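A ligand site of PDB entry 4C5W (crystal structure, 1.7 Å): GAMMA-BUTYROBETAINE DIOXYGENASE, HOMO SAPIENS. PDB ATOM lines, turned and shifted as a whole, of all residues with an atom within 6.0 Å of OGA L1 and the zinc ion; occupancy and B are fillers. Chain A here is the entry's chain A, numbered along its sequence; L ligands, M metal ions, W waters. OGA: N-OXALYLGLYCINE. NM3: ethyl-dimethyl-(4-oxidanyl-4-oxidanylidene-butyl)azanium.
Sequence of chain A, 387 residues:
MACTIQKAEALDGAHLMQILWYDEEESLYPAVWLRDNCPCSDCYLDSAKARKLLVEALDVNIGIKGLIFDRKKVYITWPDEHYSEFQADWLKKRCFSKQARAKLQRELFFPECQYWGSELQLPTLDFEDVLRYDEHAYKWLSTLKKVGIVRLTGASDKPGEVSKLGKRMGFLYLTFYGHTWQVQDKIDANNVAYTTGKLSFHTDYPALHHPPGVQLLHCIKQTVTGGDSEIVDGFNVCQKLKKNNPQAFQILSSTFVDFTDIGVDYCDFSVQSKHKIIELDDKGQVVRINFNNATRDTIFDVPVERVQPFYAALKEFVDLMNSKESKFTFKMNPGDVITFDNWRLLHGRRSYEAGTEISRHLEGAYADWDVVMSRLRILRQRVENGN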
ATOM      1  N   TRP A 181      30.249   4.913  -4.842  1.00  0.00           N
ATOM      2  CA  TRP A 181      30.148   4.008  -3.724  1.00  0.00           C
ATOM      3  C   TRP A 181      30.233   2.570  -4.199  1.00  0.00           C
ATOM      4  O   TRP A 181      29.953   2.275  -5.384  1.00  0.00           O
ATOM      5  CB  TRP A 181      28.896   4.251  -2.877  1.00  0.00           C
ATOM      6  CG  TRP A 181      27.756   4.848  -3.617  1.00  0.00           C
ATOM      7  CD1 TRP A 181      27.432   6.169  -3.679  1.00  0.00           C
ATOM      8  CD2 TRP A 181      26.821   4.160  -4.454  1.00  0.00           C
ATOM      9  NE1 TRP A 181      26.348   6.351  -4.479  1.00  0.00           N
ATOM     10  CE2 TRP A 181      25.941   5.142  -4.976  1.00  0.00           C
ATOM     11  CE3 TRP A 181      26.612   2.810  -4.784  1.00  0.00           C
ATOM     12  CZ2 TRP A 181      24.891   4.812  -5.825  1.00  0.00           C
ATOM     13  CZ3 TRP A 181      25.578   2.488  -5.607  1.00  0.00           C
ATOM     14  CH2 TRP A 181      24.705   3.490  -6.120  1.00  0.00           C
ATOM     15  N   VAL A 183      29.148  -1.273  -3.956  1.00  0.00           N
ATOM     16  CA  VAL A 183      28.144  -2.247  -3.568  1.00  0.00           C
ATOM     17  C   VAL A 183      28.848  -3.590  -3.456  1.00  0.00           C
ATOM     18  O   VAL A 183      29.171  -4.220  -4.445  1.00  0.00           O
ATOM     19  CB  VAL A 183      26.967  -2.319  -4.554  1.00  0.00           C
ATOM     20  CG1 VAL A 183      25.914  -3.250  -4.019  1.00  0.00           C
ATOM     21  CG2 VAL A 183      26.412  -0.915  -4.813  1.00  0.00           C
ATOM     22  N   ASN A 191      24.232  -0.320   5.529  1.00  0.00           N
ATOM     23  CA  ASN A 191      23.102  -0.295   4.611  1.00  0.00           C
ATOM     24  C   ASN A 191      22.837  -1.723   4.138  1.00  0.00           C
ATOM     25  O   ASN A 191      23.778  -2.458   3.906  1.00  0.00           O
ATOM     26  CB  ASN A 191      23.446   0.626   3.429  1.00  0.00           C
ATOM     27  CG  ASN A 191      22.225   0.996   2.578  1.00  0.00           C
ATOM     28  OD1 ASN A 191      21.729   0.193   1.799  1.00  0.00           O
ATOM     29  ND2 ASN A 191      21.747   2.216   2.734  1.00  0.00           N
ATOM     30  N   ALA A 193      22.016  -2.729   1.338  1.00  0.00           N
ATOM     31  CA  ALA A 193      22.668  -2.918   0.037  1.00  0.00           C
ATOM     32  C   ALA A 193      24.058  -3.569   0.132  1.00  0.00           C
ATOM     33  O   ALA A 193      24.482  -4.346  -0.735  1.00  0.00           O
ATOM     34  CB  ALA A 193      22.771  -1.592  -0.693  1.00  0.00           C
ATOM     35  N   TYR A 194      24.748  -3.268   1.222  1.00  0.00           N
ATOM     36  CA  TYR A 194      26.117  -3.728   1.418  1.00  0.00           C
ATOM     37  C   TYR A 194      26.165  -5.072   2.185  1.00  0.00           C
ATOM     38  O   TYR A 194      26.996  -5.290   3.055  1.00  0.00           O
ATOM     39  CB  TYR A 194      26.887  -2.660   2.159  1.00  0.00           C
ATOM     40  CG  TYR A 194      26.985  -1.304   1.456  1.00  0.00           C
ATOM     41  CD1 TYR A 194      26.927  -1.192   0.057  1.00  0.00           C
ATOM     42  CD2 TYR A 194      27.206  -0.154   2.192  1.00  0.00           C
ATOM     43  CE1 TYR A 194      27.051   0.043  -0.572  1.00  0.00           C
ATOM     44  CE2 TYR A 194      27.313   1.091   1.573  1.00  0.00           C
ATOM     45  CZ  TYR A 194      27.250   1.174   0.188  1.00  0.00           C
ATOM     46  OH  TYR A 194      27.377   2.378  -0.432  1.00  0.00           O
ATOM     47  N   LEU A 199      17.487  -7.728  -2.420  1.00  0.00           N
ATOM     48  CA  LEU A 199      16.840  -6.418  -2.358  1.00  0.00           C
ATOM     49  C   LEU A 199      15.583  -6.506  -3.167  1.00  0.00           C
ATOM     50  O   LEU A 199      15.631  -6.770  -4.374  1.00  0.00           O
ATOM     51  CB  LEU A 199      17.779  -5.331  -2.923  1.00  0.00           C
ATOM     52  CG  LEU A 199      19.145  -5.200  -2.248  1.00  0.00           C
ATOM     53  CD1 LEU A 199      19.930  -4.084  -2.895  1.00  0.00           C
ATOM     54  CD2 LEU A 199      18.981  -4.938  -0.749  1.00  0.00           C
ATOM     55  N   HIS A 202      12.868  -1.322  -4.994  1.00  0.00           N
ATOM     56  CA  HIS A 202      12.934  -0.053  -4.313  1.00  0.00           C
ATOM     57  C   HIS A 202      13.454   1.018  -5.257  1.00  0.00           C
ATOM     58  O   HIS A 202      14.034   0.703  -6.297  1.00  0.00           O
ATOM     59  CB  HIS A 202      13.922  -0.159  -3.137  1.00  0.00           C
ATOM     60  CG  HIS A 202      15.329  -0.432  -3.553  1.00  0.00           C
ATOM     61  ND1 HIS A 202      15.755  -1.679  -3.947  1.00  0.00           N
ATOM     62  CD2 HIS A 202      16.423   0.376  -3.603  1.00  0.00           C
ATOM     63  CE1 HIS A 202      17.050  -1.624  -4.249  1.00  0.00           C
ATOM     64  NE2 HIS A 202      17.466  -0.386  -4.049  1.00  0.00           N
ATOM     65  N   THR A 203      13.250   2.272  -4.845  1.00  0.00           N
ATOM     66  CA  THR A 203      13.971   3.432  -5.370  1.00  0.00           C
ATOM     67  C   THR A 203      15.080   3.729  -4.382  1.00  0.00           C
ATOM     68  O   THR A 203      14.924   3.398  -3.200  1.00  0.00           O
ATOM     69  CB  THR A 203      13.046   4.668  -5.528  1.00  0.00           C
ATOM     70  OG1 THR A 203      12.472   5.012  -4.269  1.00  0.00           O
ATOM     71  CG2 THR A 203      11.913   4.372  -6.478  1.00  0.00           C
ATOM     72  N   ASP A 204      16.175   4.326  -4.837  1.00  0.00           N
ATOM     73  CA  ASP A 204      17.253   4.695  -3.945  1.00  0.00           C
ATOM     74  C   ASP A 204      16.994   6.043  -3.286  1.00  0.00           C
ATOM     75  O   ASP A 204      16.540   7.010  -3.914  1.00  0.00           O
ATOM     76  CB  ASP A 204      18.600   4.757  -4.664  1.00  0.00           C
ATOM     77  CG  ASP A 204      19.334   3.422  -4.697  1.00  0.00           C
ATOM     78  OD1 ASP A 204      18.686   2.358  -4.716  1.00  0.00           O
ATOM     79  OD2 ASP A 204      20.599   3.409  -4.715  1.00  0.00           O
ATOM     80  N   GLN A 215      20.496   7.035 -11.602  1.00  0.00           N
ATOM     81  CA  GLN A 215      21.452   6.169 -10.947  1.00  0.00           C
ATOM     82  C   GLN A 215      22.332   5.456 -11.995  1.00  0.00           C
ATOM     83  O   GLN A 215      21.872   5.041 -13.041  1.00  0.00           O
ATOM     84  CB  GLN A 215      20.702   5.142 -10.096  1.00  0.00           C
ATOM     85  CG  GLN A 215      21.620   4.157  -9.376  1.00  0.00           C
ATOM     86  CD  GLN A 215      20.940   3.366  -8.278  1.00  0.00           C
ATOM     87  OE1 GLN A 215      21.444   2.316  -7.848  1.00  0.00           O
ATOM     88  NE2 GLN A 215      19.814   3.853  -7.826  1.00  0.00           N
ATOM     89  N   LEU A 217      25.101   2.210 -12.215  1.00  0.00           N
ATOM     90  CA  LEU A 217      25.665   1.026 -11.556  1.00  0.00           C
ATOM     91  C   LEU A 217      26.543   0.273 -12.546  1.00  0.00           C
ATOM     92  O   LEU A 217      26.079  -0.171 -13.578  1.00  0.00           O
ATOM     93  CB  LEU A 217      24.571   0.068 -11.067  1.00  0.00           C
ATOM     94  CG  LEU A 217      23.763   0.316  -9.798  1.00  0.00           C
ATOM     95  CD1 LEU A 217      22.730  -0.805  -9.598  1.00  0.00           C
ATOM     96  CD2 LEU A 217      24.706   0.383  -8.636  1.00  0.00           C
ATOM     97  N   GLY A 227      22.561 -12.844  -7.442  1.00  0.00           N
ATOM     98  CA  GLY A 227      22.881 -11.461  -7.763  1.00  0.00           C
ATOM     99  C   GLY A 227      22.316 -10.938  -9.052  1.00  0.00           C
ATOM    100  O   GLY A 227      22.758  -9.912  -9.542  1.00  0.00           O
ATOM    101  N   ASP A 228      21.298 -11.631  -9.582  1.00  0.00           N
ATOM    102  CA  ASP A 228      20.583 -11.139 -10.770  1.00  0.00           C
ATOM    103  C   ASP A 228      19.902  -9.808 -10.476  1.00  0.00           C
ATOM    104  O   ASP A 228      19.474  -9.571  -9.332  1.00  0.00           O
ATOM    105  CB  ASP A 228      19.508 -12.139 -11.229  1.00  0.00           C
ATOM    106  CG  ASP A 228      20.039 -13.532 -11.435  1.00  0.00           C
ATOM    107  OD1 ASP A 228      20.364 -14.162 -10.414  1.00  0.00           O
ATOM    108  OD2 ASP A 228      20.125 -13.979 -12.601  1.00  0.00           O
ATOM    109  N   SER A 229      19.764  -8.969 -11.498  1.00  0.00           N
ATOM    110  CA  SER A 229      19.062  -7.696 -11.369  1.00  0.00           C
ATOM    111  C   SER A 229      17.606  -7.832 -11.825  1.00  0.00           C
ATOM    112  O   SER A 229      17.274  -8.665 -12.659  1.00  0.00           O
ATOM    113  CB  SER A 229      19.733  -6.634 -12.218  1.00  0.00           C
ATOM    114  OG  SER A 229      21.047  -6.429 -11.790  1.00  0.00           O
ATOM    115  N   ASN A 292      11.637   2.740  -0.428  1.00  0.00           N
ATOM    116  CA  ASN A 292      12.648   1.750  -0.114  1.00  0.00           C
ATOM    117  C   ASN A 292      12.257   1.112   1.234  1.00  0.00           C
ATOM    118  O   ASN A 292      12.174   1.819   2.244  1.00  0.00           O
ATOM    119  CB  ASN A 292      14.040   2.360  -0.059  1.00  0.00           C
ATOM    120  CG  ASN A 292      15.152   1.334   0.192  1.00  0.00           C
ATOM    121  OD1 ASN A 292      14.902   0.177   0.549  1.00  0.00           O
ATOM    122  ND2 ASN A 292      16.371   1.754   0.019  1.00  0.00           N
ATOM    123  N   MET A 332      23.898  -8.620 -14.735  1.00  0.00           N
ATOM    124  CA  MET A 332      25.021  -7.804 -15.164  1.00  0.00           C
ATOM    125  C   MET A 332      26.281  -8.649 -15.207  1.00  0.00           C
ATOM    126  O   MET A 332      26.511  -9.483 -14.322  1.00  0.00           O
ATOM    127  CB  MET A 332      25.208  -6.632 -14.196  1.00  0.00           C
ATOM    128  CG  MET A 332      23.959  -5.768 -14.042  1.00  0.00           C
ATOM    129  SD  MET A 332      24.360  -4.218 -13.203  1.00  0.00           S
ATOM    130  CE  MET A 332      25.293  -3.432 -14.500  1.00  0.00           C
ATOM    131  N   PHE A 340      19.842   4.526 -15.081  1.00  0.00           N
ATOM    132  CA  PHE A 340      18.381   4.511 -15.075  1.00  0.00           C
ATOM    133  C   PHE A 340      17.776   5.649 -14.272  1.00  0.00           C
ATOM    134  O   PHE A 340      18.456   6.301 -13.445  1.00  0.00           O
ATOM    135  CB  PHE A 340      17.853   3.130 -14.616  1.00  0.00           C
ATOM    136  CG  PHE A 340      18.313   2.693 -13.237  1.00  0.00           C
ATOM    137  CD1 PHE A 340      19.502   1.973 -13.080  1.00  0.00           C
ATOM    138  CD2 PHE A 340      17.563   2.978 -12.107  1.00  0.00           C
ATOM    139  CE1 PHE A 340      19.929   1.549 -11.833  1.00  0.00           C
ATOM    140  CE2 PHE A 340      17.972   2.535 -10.850  1.00  0.00           C
ATOM    141  CZ  PHE A 340      19.152   1.835 -10.710  1.00  0.00           C
ATOM    142  N   HIS A 347      14.081  -0.974  -8.663  1.00  0.00           N
ATOM    143  CA  HIS A 347      15.083  -1.984  -9.000  1.00  0.00           C
ATOM    144  C   HIS A 347      15.325  -2.879  -7.820  1.00  0.00           C
ATOM    145  O   HIS A 347      15.003  -2.529  -6.667  1.00  0.00           O
ATOM    146  CB  HIS A 347      16.399  -1.320  -9.481  1.00  0.00           C
ATOM    147  CG  HIS A 347      17.073  -0.446  -8.455  1.00  0.00           C
ATOM    148  ND1 HIS A 347      16.626   0.812  -8.154  1.00  0.00           N
ATOM    149  CD2 HIS A 347      18.158  -0.669  -7.669  1.00  0.00           C
ATOM    150  CE1 HIS A 347      17.416   1.348  -7.233  1.00  0.00           C
ATOM    151  NE2 HIS A 347      18.331   0.453  -6.894  1.00  0.00           N
ATOM    152  N   GLY A 348      15.909  -4.035  -8.097  1.00  0.00           N
ATOM    153  CA  GLY A 348      16.207  -4.973  -7.034  1.00  0.00           C
ATOM    154  C   GLY A 348      17.299  -5.928  -7.459  1.00  0.00           C
ATOM    155  O   GLY A 348      17.789  -5.887  -8.584  1.00  0.00           O
ATOM    156  N   ARG A 349      17.621  -6.827  -6.551  1.00  0.00           N
ATOM    157  CA  ARG A 349      18.654  -7.789  -6.764  1.00  0.00           C
ATOM    158  C   ARG A 349      18.302  -9.090  -6.022  1.00  0.00           C
ATOM    159  O   ARG A 349      17.796  -9.060  -4.909  1.00  0.00           O
ATOM    160  CB  ARG A 349      19.939  -7.212  -6.188  1.00  0.00           C
ATOM    161  CG  ARG A 349      20.918  -8.230  -5.693  1.00  0.00           C
ATOM    162  CD  ARG A 349      22.014  -7.572  -4.895  1.00  0.00           C
ATOM    163  NE  ARG A 349      21.819  -7.609  -3.457  1.00  0.00           N
ATOM    164  CZ  ARG A 349      22.460  -6.804  -2.613  1.00  0.00           C
ATOM    165  NH1 ARG A 349      23.310  -5.862  -3.060  1.00  0.00           N
ATOM    166  NH2 ARG A 349      22.241  -6.911  -1.304  1.00  0.00           N
ATOM    167  N   ARG A 360      31.469 -10.254  -5.480  1.00  0.00           N
ATOM    168  CA  ARG A 360      30.556  -9.390  -6.220  1.00  0.00           C
ATOM    169  C   ARG A 360      30.808  -7.942  -5.808  1.00  0.00           C
ATOM    170  O   ARG A 360      30.914  -7.627  -4.622  1.00  0.00           O
ATOM    171  CB  ARG A 360      29.109  -9.767  -5.942  1.00  0.00           C
ATOM    172  CG  ARG A 360      28.121  -9.109  -6.900  1.00  0.00           C
ATOM    173  CD  ARG A 360      26.716  -9.498  -6.496  1.00  0.00           C
ATOM    174  NE  ARG A 360      25.678  -9.048  -7.420  1.00  0.00           N
ATOM    175  CZ  ARG A 360      25.022  -7.888  -7.357  1.00  0.00           C
ATOM    176  NH1 ARG A 360      25.338  -6.984  -6.442  1.00  0.00           N
ATOM    177  NH2 ARG A 360      24.070  -7.623  -8.257  1.00  0.00           N
ATOM    178  N   LEU A 362      29.792  -3.898  -7.370  1.00  0.00           N
ATOM    179  CA  LEU A 362      29.366  -2.852  -8.269  1.00  0.00           C
ATOM    180  C   LEU A 362      29.891  -1.510  -7.745  1.00  0.00           C
ATOM    181  O   LEU A 362      29.989  -1.304  -6.523  1.00  0.00           O
ATOM    182  CB  LEU A 362      27.845  -2.804  -8.388  1.00  0.00           C
ATOM    183  CG  LEU A 362      27.050  -4.090  -8.395  1.00  0.00           C
ATOM    184  CD1 LEU A 362      25.566  -3.764  -8.422  1.00  0.00           C
ATOM    185  CD2 LEU A 362      27.448  -4.936  -9.589  1.00  0.00           C
ATOM    186  N   TYR A 366      25.218   8.727  -8.519  1.00  0.00           N
ATOM    187  CA  TYR A 366      23.961   9.371  -8.801  1.00  0.00           C
ATOM    188  C   TYR A 366      24.197  10.639  -9.614  1.00  0.00           C
ATOM    189  O   TYR A 366      25.268  11.258  -9.550  1.00  0.00           O
ATOM    190  CB  TYR A 366      23.304   9.771  -7.489  1.00  0.00           C
ATOM    191  CG  TYR A 366      22.920   8.622  -6.583  1.00  0.00           C
ATOM    192  CD1 TYR A 366      22.049   7.620  -7.015  1.00  0.00           C
ATOM    193  CD2 TYR A 366      23.368   8.597  -5.265  1.00  0.00           C
ATOM    194  CE1 TYR A 366      21.686   6.590  -6.164  1.00  0.00           C
ATOM    195  CE2 TYR A 366      22.986   7.588  -4.426  1.00  0.00           C
ATOM    196  CZ  TYR A 366      22.155   6.584  -4.869  1.00  0.00           C
ATOM    197  OH  TYR A 366      21.793   5.574  -3.960  1.00  0.00           O
HETATM  198  C1  OGA L   1      21.595  -0.655  -4.206  1.00  0.00           C
HETATM  199  C2  OGA L   1      21.213  -1.626  -5.224  1.00  0.00           C
HETATM  200  C4  OGA L   1      21.641  -3.465  -6.716  1.00  0.00           C
HETATM  201  C5  OGA L   1      22.602  -4.632  -6.834  1.00  0.00           C
HETATM  202  O1  OGA L   1      22.743  -0.742  -3.734  1.00  0.00           O
HETATM  203  O2  OGA L   1      20.757   0.245  -3.879  1.00  0.00           O
HETATM  204  O2' OGA L   1      20.095  -1.541  -5.667  1.00  0.00           O
HETATM  205  O3  OGA L   1      22.506  -5.289  -7.874  1.00  0.00           O
HETATM  206  N1  OGA L   1      22.054  -2.556  -5.660  1.00  0.00           N
HETATM  207  O4  OGA L   1      23.428  -4.890  -5.892  1.00  0.00           O
HETATM  208  N1  NM3 L   2      23.393   3.059  -1.448  1.00  0.00           N
HETATM  209  C8  NM3 L   2      23.829   2.574  -0.103  1.00  0.00           C
HETATM  210  O4  NM3 L   2      17.934   4.178  -0.013  1.00  0.00           O
HETATM  211  C5  NM3 L   2      19.049   3.613   0.065  1.00  0.00           C
HETATM  212  O7  NM3 L   2      19.720   3.544   1.118  1.00  0.00           O
HETATM  213  C6  NM3 L   2      19.509   2.924  -1.196  1.00  0.00           C
HETATM  214  C2  NM3 L   2      21.963   3.483  -1.375  1.00  0.00           C
HETATM  215  C9  NM3 L   2      24.191   4.244  -1.867  1.00  0.00           C
HETATM  216  C10 NM3 L   2      23.624   1.993  -2.431  1.00  0.00           C
HETATM  217  C3  NM3 L   2      20.946   2.380  -1.149  1.00  0.00           C
HETATM  218 ZN    ZN M   1      19.137   0.388  -4.999  1.00  0.00          ZN
HETATM  219  O   HOH W   1      20.513  -4.984  -9.663  1.00  0.00           O
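Within 4 Å of the zinc ion: His 202, Asp 204 and His 347. The nearest printed residue that does not touch the zinc ion is Gln 215 (4.1 Å).
The zinc ion is bound by O2 of OGA L1 (2.0 Å), OD1 of Asp 204 (2.0 Å), NE2 of His 347 (2.1 Å), NE2 of His 202 (2.1 Å) and O2' of OGA L1 (2.3 Å).
NE2 of Gln 215 sits close to OD2 of Asp 204 (3.2 Å). OD2 of Asp 204 lies within hydrogen-bond range of OH of Tyr 366, 2.6 Å away. NH2 of Arg 360 is in hydrogen-bond range of O of Gly 227, at 2.9 Å. NH1 of Arg 349 is in hydrogen-bond range of O of Ala 193. The backbone carbonyl oxygen of Arg 349 is in hydrogen-bond range of the backbone NH of Leu 199 (2.8 Å). The backbone NH (N) of Ala 193 sits at hydrogen-bond distance from the side-chain amide oxygen (OD1) of Asn 191, 3.0 Å away. The backbone carbonyl oxygen of Leu 362 is in hydrogen-bond range of the backbone NH of Val 183.
Merely in contact with OGA L1: Val 183, Ala 193, Leu 199 and Leu 362. Hydrophobic or aromatic side chains within 4 Å of OGA L1: Val 183, Ala 193, Leu 199, His 202, His 347 and Leu 362. Of the 23 residues printed, 9 come within 4 Å of OGA L1.
An oxygen (O3) of OGA L1 lies within salt-bridge range of the guanidinium group (NH2) of Arg 360 (2.8 Å). An oxygen (O4) of OGA L1 lies within salt-bridge range of the guanidinium group of Arg 349 (3.0 Å). ND2 of Asn 191 lies within hydrogen-bond range of O7 of NM3 L2, 2.9 Å away. The side-chain amide nitrogen of Asn 292 sits at hydrogen-bond distance from an oxygen (O4) of NM3 L2 (2.9 Å).
Water W1 lies within hydrogen-bond range of OG of Ser 229, O3 of OGA L1 and O of Gly 348.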
